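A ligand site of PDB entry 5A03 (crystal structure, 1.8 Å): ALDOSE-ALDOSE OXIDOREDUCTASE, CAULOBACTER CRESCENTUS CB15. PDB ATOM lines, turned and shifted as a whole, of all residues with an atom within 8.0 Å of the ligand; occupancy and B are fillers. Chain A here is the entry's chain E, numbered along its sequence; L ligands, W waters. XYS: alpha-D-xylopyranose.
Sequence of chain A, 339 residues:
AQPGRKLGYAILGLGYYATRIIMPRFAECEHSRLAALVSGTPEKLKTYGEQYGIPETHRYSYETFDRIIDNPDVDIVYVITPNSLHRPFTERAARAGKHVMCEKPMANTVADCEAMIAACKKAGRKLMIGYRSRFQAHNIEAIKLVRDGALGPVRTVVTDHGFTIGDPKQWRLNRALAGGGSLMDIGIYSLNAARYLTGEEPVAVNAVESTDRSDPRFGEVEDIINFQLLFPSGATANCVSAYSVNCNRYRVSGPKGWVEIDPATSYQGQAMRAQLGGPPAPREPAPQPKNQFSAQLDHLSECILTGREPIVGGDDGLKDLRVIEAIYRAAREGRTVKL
The side-chain amide nitrogen (NE2) of Gln 136 lies within hydrogen-bond range of a ring nitrogen (ND1) of His 138.
A ring nitrogen (NE2) of His 138 is in hydrogen-bond range of the backbone carbonyl oxygen of Gln 270 (3.3 Å).
NE of Arg 283 lies within salt-bridge range of OE2 of Glu 141 (2.7 Å).
The backbone NH of Arg 283 lies within hydrogen-bond range of the backbone carbonyl oxygen of Met 272 (3.1 Å).
The backbone carbonyl oxygen (O) of Ala 271 sits at hydrogen-bond distance from the backbone NH (N) of Asp 262, at 3.0 Å.
The backbone carbonyl oxygen of Arg 283 lies within hydrogen-bond range of an oxygen (O4) of the ligand (2.8 Å).
NE2 of His 138 sits at hydrogen-bond distance from O3 of the ligand (2.9 Å).
An oxygen (O3) of the ligand sits at hydrogen-bond distance from the side-chain carboxylate (OE1) of Glu 284, 3.2 Å away.
N of Met 272 sits at hydrogen-bond distance from O4 of the ligand (2.9 Å).
Water W1 lies within hydrogen-bond range of the backbone carbonyl oxygen of Gly 269, the backbone carbonyl oxygen of Gln 270 and an oxygen (O2) of the ligand.
O of Gln 270 touches C3 of the ligand, at 3.7 Å.
Ala 271 touches the ligand (CB to O1, 3.6 Å).
Hydrophobic or aromatic side chains within 4 Å of the ligand: His 138, Ala 271 and Met 272.
Within 4 Å of the ligand: His 138, Gln 270, Ala 271, Met 272, Arg 283 and Glu 284.
The nearest printed residue that does not touch the ligand is Pro 285 (4.1 Å).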
ATOM      1  N   GLN A 136       0.191  23.038 -22.199  1.00  0.00           N
ATOM      2  CA  GLN A 136      -0.350  21.939 -21.401  1.00  0.00           C
ATOM      3  C   GLN A 136       0.704  20.821 -21.310  1.00  0.00           C
ATOM      4  O   GLN A 136       1.310  20.476 -22.315  1.00  0.00           O
ATOM      5  CB  GLN A 136      -1.668  21.463 -22.030  1.00  0.00           C
ATOM      6  CG  GLN A 136      -2.565  20.631 -21.128  1.00  0.00           C
ATOM      7  CD  GLN A 136      -2.103  19.192 -21.042  1.00  0.00           C
ATOM      8  OE1 GLN A 136      -1.588  18.637 -22.026  1.00  0.00           O
ATOM      9  NE2 GLN A 136      -2.262  18.582 -19.872  1.00  0.00           N
ATOM     10  N   ALA A 137       0.916  20.271 -20.111  1.00  0.00           N
ATOM     11  CA  ALA A 137       2.085  19.421 -19.862  1.00  0.00           C
ATOM     12  C   ALA A 137       2.206  18.224 -20.812  1.00  0.00           C
ATOM     13  O   ALA A 137       3.283  17.962 -21.343  1.00  0.00           O
ATOM     14  CB  ALA A 137       2.083  18.922 -18.399  1.00  0.00           C
ATOM     15  N   HIS A 138       1.096  17.519 -21.028  1.00  0.00           N
ATOM     16  CA  HIS A 138       1.119  16.299 -21.839  1.00  0.00           C
ATOM     17  C   HIS A 138       1.410  16.640 -23.306  1.00  0.00           C
ATOM     18  O   HIS A 138       2.150  15.917 -23.996  1.00  0.00           O
ATOM     19  CB  HIS A 138      -0.214  15.542 -21.713  1.00  0.00           C
ATOM     20  CG  HIS A 138      -0.537  15.084 -20.316  1.00  0.00           C
ATOM     21  ND1 HIS A 138      -0.929  15.953 -19.318  1.00  0.00           N
ATOM     22  CD2 HIS A 138      -0.554  13.843 -19.759  1.00  0.00           C
ATOM     23  CE1 HIS A 138      -1.160  15.267 -18.206  1.00  0.00           C
ATOM     24  NE2 HIS A 138      -0.935  13.994 -18.446  1.00  0.00           N
ATOM     25  N   GLU A 141       5.018  17.414 -23.699  1.00  0.00           N
ATOM     26  CA  GLU A 141       5.771  16.162 -23.635  1.00  0.00           C
ATOM     27  C   GLU A 141       5.737  15.424 -24.973  1.00  0.00           C
ATOM     28  O   GLU A 141       6.743  14.871 -25.409  1.00  0.00           O
ATOM     29  CB  GLU A 141       5.218  15.272 -22.516  1.00  0.00           C
ATOM     30  CG  GLU A 141       5.861  13.894 -22.399  1.00  0.00           C
ATOM     31  CD  GLU A 141       7.159  13.895 -21.600  1.00  0.00           C
ATOM     32  OE1 GLU A 141       7.568  14.959 -21.053  1.00  0.00           O
ATOM     33  OE2 GLU A 141       7.773  12.813 -21.511  1.00  0.00           O
ATOM     34  N   GLU A 260       0.382   8.770 -27.529  1.00  0.00           N
ATOM     35  CA  GLU A 260      -0.978   9.277 -27.674  1.00  0.00           C
ATOM     36  C   GLU A 260      -1.466   9.920 -26.381  1.00  0.00           C
ATOM     37  O   GLU A 260      -0.964   9.621 -25.290  1.00  0.00           O
ATOM     38  CB  GLU A 260      -1.936   8.161 -28.109  1.00  0.00           C
ATOM     39  CG  GLU A 260      -2.220   7.138 -27.009  1.00  0.00           C
ATOM     40  CD  GLU A 260      -3.039   5.948 -27.486  1.00  0.00           C
ATOM     41  OE1 GLU A 260      -3.366   5.853 -28.699  1.00  0.00           O
ATOM     42  OE2 GLU A 260      -3.347   5.070 -26.637  1.00  0.00           O
ATOM     43  N   ILE A 261      -2.422  10.821 -26.518  1.00  0.00           N
ATOM     44  CA  ILE A 261      -3.063  11.462 -25.376  1.00  0.00           C
ATOM     45  C   ILE A 261      -4.559  11.410 -25.628  1.00  0.00           C
ATOM     46  O   ILE A 261      -5.021  11.743 -26.731  1.00  0.00           O
ATOM     47  CB  ILE A 261      -2.608  12.931 -25.173  1.00  0.00           C
ATOM     48  CG1 ILE A 261      -1.124  13.112 -25.518  1.00  0.00           C
ATOM     49  CG2 ILE A 261      -2.873  13.397 -23.722  1.00  0.00           C
ATOM     50  CD1 ILE A 261      -0.663  14.600 -25.516  1.00  0.00           C
ATOM     51  N   ASP A 262      -5.301  10.965 -24.632  1.00  0.00           N
ATOM     52  CA  ASP A 262      -6.755  10.830 -24.719  1.00  0.00           C
ATOM     53  C   ASP A 262      -7.324  10.905 -23.297  1.00  0.00           C
ATOM     54  O   ASP A 262      -7.184   9.944 -22.550  1.00  0.00           O
ATOM     55  CB  ASP A 262      -7.129   9.484 -25.378  1.00  0.00           C
ATOM     56  CG  ASP A 262      -8.597   9.368 -25.707  1.00  0.00           C
ATOM     57  OD1 ASP A 262      -9.364  10.300 -25.398  1.00  0.00           O
ATOM     58  OD2 ASP A 262      -8.998   8.325 -26.300  1.00  0.00           O
ATOM     59  N   PRO A 263      -7.978  12.030 -22.942  1.00  0.00           N
ATOM     60  CA  PRO A 263      -8.197  13.230 -23.772  1.00  0.00           C
ATOM     61  C   PRO A 263      -6.916  14.030 -23.989  1.00  0.00           C
ATOM     62  O   PRO A 263      -6.057  14.029 -23.119  1.00  0.00           O
ATOM     63  CB  PRO A 263      -9.214  14.050 -22.959  1.00  0.00           C
ATOM     64  CG  PRO A 263      -8.966  13.627 -21.523  1.00  0.00           C
ATOM     65  CD  PRO A 263      -8.649  12.142 -21.622  1.00  0.00           C
ATOM     66  N   GLY A 269      -7.734  16.489 -17.318  1.00  0.00           N
ATOM     67  CA  GLY A 269      -7.978  15.057 -17.474  1.00  0.00           C
ATOM     68  C   GLY A 269      -7.084  14.335 -18.466  1.00  0.00           C
ATOM     69  O   GLY A 269      -7.268  13.136 -18.690  1.00  0.00           O
ATOM     70  N   GLN A 270      -6.111  15.043 -19.041  1.00  0.00           N
ATOM     71  CA  GLN A 270      -5.186  14.449 -20.011  1.00  0.00           C
ATOM     72  C   GLN A 270      -4.554  13.166 -19.488  1.00  0.00           C
ATOM     73  O   GLN A 270      -4.120  13.101 -18.338  1.00  0.00           O
ATOM     74  CB  GLN A 270      -4.077  15.425 -20.387  1.00  0.00           C
ATOM     75  CG  GLN A 270      -4.435  16.356 -21.539  1.00  0.00           C
ATOM     76  CD  GLN A 270      -5.277  17.546 -21.102  1.00  0.00           C
ATOM     77  OE1 GLN A 270      -5.732  17.635 -19.947  1.00  0.00           O
ATOM     78  NE2 GLN A 270      -5.480  18.488 -22.017  1.00  0.00           N
ATOM     79  N   ALA A 271      -4.480  12.154 -20.351  1.00  0.00           N
ATOM     80  CA  ALA A 271      -3.792  10.910 -20.026  1.00  0.00           C
ATOM     81  C   ALA A 271      -2.961  10.464 -21.215  1.00  0.00           C
ATOM     82  O   ALA A 271      -3.476  10.346 -22.327  1.00  0.00           O
ATOM     83  CB  ALA A 271      -4.792   9.823 -19.628  1.00  0.00           C
ATOM     84  N   MET A 272      -1.667  10.239 -20.998  1.00  0.00           N
ATOM     85  CA  MET A 272      -0.763   9.863 -22.058  1.00  0.00           C
ATOM     86  C   MET A 272      -0.382   8.391 -22.000  1.00  0.00           C
ATOM     87  O   MET A 272      -0.153   7.839 -20.916  1.00  0.00           O
ATOM     88  CB  MET A 272       0.495  10.732 -22.010  1.00  0.00           C
ATOM     89  CG  MET A 272       1.612  10.289 -22.937  1.00  0.00           C
ATOM     90  SD  MET A 272       3.052  11.358 -22.874  1.00  0.00           S
ATOM     91  CE  MET A 272       2.500  12.754 -23.896  1.00  0.00           C
ATOM     92  N   ARG A 273      -0.312   7.752 -23.161  1.00  0.00           N
ATOM     93  CA  ARG A 273       0.176   6.380 -23.266  1.00  0.00           C
ATOM     94  C   ARG A 273       1.191   6.353 -24.406  1.00  0.00           C
ATOM     95  O   ARG A 273       0.953   6.960 -25.466  1.00  0.00           O
ATOM     96  CB  ARG A 273      -0.967   5.396 -23.520  1.00  0.00           C
ATOM     97  CG  ARG A 273      -0.529   3.928 -23.565  1.00  0.00           C
ATOM     98  CD  ARG A 273      -1.728   2.986 -23.653  1.00  0.00           C
ATOM     99  NE  ARG A 273      -2.415   3.078 -24.936  1.00  0.00           N
ATOM    100  CZ  ARG A 273      -2.927   2.033 -25.599  1.00  0.00           C
ATOM    101  NH1 ARG A 273      -2.825   0.806 -25.104  1.00  0.00           N
ATOM    102  NH2 ARG A 273      -3.541   2.239 -26.763  1.00  0.00           N
ATOM    103  N   ALA A 281       2.487   1.750 -22.592  1.00  0.00           N
ATOM    104  CA  ALA A 281       2.540   1.979 -21.154  1.00  0.00           C
ATOM    105  C   ALA A 281       2.207   3.432 -20.847  1.00  0.00           C
ATOM    106  O   ALA A 281       2.466   4.312 -21.663  1.00  0.00           O
ATOM    107  CB  ALA A 281       3.929   1.632 -20.619  1.00  0.00           C
ATOM    108  N   PRO A 282       1.624   3.679 -19.660  1.00  0.00           N
ATOM    109  CA  PRO A 282       1.363   5.066 -19.257  1.00  0.00           C
ATOM    110  C   PRO A 282       2.650   5.869 -19.236  1.00  0.00           C
ATOM    111  O   PRO A 282       3.712   5.316 -18.973  1.00  0.00           O
ATOM    112  CB  PRO A 282       0.772   4.928 -17.847  1.00  0.00           C
ATOM    113  CG  PRO A 282       0.243   3.518 -17.786  1.00  0.00           C
ATOM    114  CD  PRO A 282       1.169   2.700 -18.648  1.00  0.00           C
ATOM    115  N   ARG A 283       2.543   7.167 -19.518  1.00  0.00           N
ATOM    116  CA  ARG A 283       3.692   8.039 -19.395  1.00  0.00           C
ATOM    117  C   ARG A 283       3.266   9.319 -18.717  1.00  0.00           C
ATOM    118  O   ARG A 283       2.292   9.944 -19.109  1.00  0.00           O
ATOM    119  CB  ARG A 283       4.315   8.340 -20.755  1.00  0.00           C
ATOM    120  CG  ARG A 283       5.564   9.199 -20.669  1.00  0.00           C
ATOM    121  CD  ARG A 283       6.256   9.332 -22.020  1.00  0.00           C
ATOM    122  NE  ARG A 283       7.484  10.121 -21.940  1.00  0.00           N
ATOM    123  CZ  ARG A 283       8.703   9.590 -21.818  1.00  0.00           C
ATOM    124  NH1 ARG A 283       8.855   8.272 -21.748  1.00  0.00           N
ATOM    125  NH2 ARG A 283       9.770  10.376 -21.757  1.00  0.00           N
ATOM    126  N   GLU A 284       4.012   9.690 -17.680  1.00  0.00           N
ATOM    127  CA  GLU A 284       3.786  10.943 -16.992  1.00  0.00           C
ATOM    128  C   GLU A 284       4.670  12.011 -17.598  1.00  0.00           C
ATOM    129  O   GLU A 284       5.877  11.832 -17.729  1.00  0.00           O
ATOM    130  CB  GLU A 284       4.067  10.784 -15.501  1.00  0.00           C
ATOM    131  CG  GLU A 284       3.055   9.897 -14.785  1.00  0.00           C
ATOM    132  CD  GLU A 284       1.799  10.651 -14.397  1.00  0.00           C
ATOM    133  OE1 GLU A 284       1.670  11.862 -14.741  1.00  0.00           O
ATOM    134  OE2 GLU A 284       0.939  10.029 -13.721  1.00  0.00           O
ATOM    135  N   PRO A 285       4.060  13.138 -17.996  1.00  0.00           N
ATOM    136  CA  PRO A 285       4.844  14.177 -18.648  1.00  0.00           C
ATOM    137  C   PRO A 285       5.691  14.958 -17.646  1.00  0.00           C
ATOM    138  O   PRO A 285       5.397  14.900 -16.448  1.00  0.00           O
ATOM    139  CB  PRO A 285       3.766  15.073 -19.290  1.00  0.00           C
ATOM    140  CG  PRO A 285       2.625  14.960 -18.368  1.00  0.00           C
ATOM    141  CD  PRO A 285       2.646  13.522 -17.851  1.00  0.00           C
HETATM  142  C1  XYS L   1      -2.591   8.837 -15.578  1.00  0.00           C
HETATM  143  C2  XYS L   1      -2.184  10.255 -15.252  1.00  0.00           C
HETATM  144  C3  XYS L   1      -1.675  10.981 -16.493  1.00  0.00           C
HETATM  145  C4  XYS L   1      -0.586  10.162 -17.193  1.00  0.00           C
HETATM  146  C5  XYS L   1      -0.970   8.688 -17.337  1.00  0.00           C
HETATM  147  O1  XYS L   1      -3.807   8.806 -16.303  1.00  0.00           O
HETATM  148  O2  XYS L   1      -3.287  10.972 -14.721  1.00  0.00           O
HETATM  149  O3  XYS L   1      -1.198  12.270 -16.150  1.00  0.00           O
HETATM  150  O4  XYS L   1      -0.299  10.715 -18.473  1.00  0.00           O
HETATM  151  O5  XYS L   1      -1.610   8.116 -16.210  1.00  0.00           O
HETATM  152  O   HOH W   1      -6.161  11.428 -16.406  1.00  0.00           O
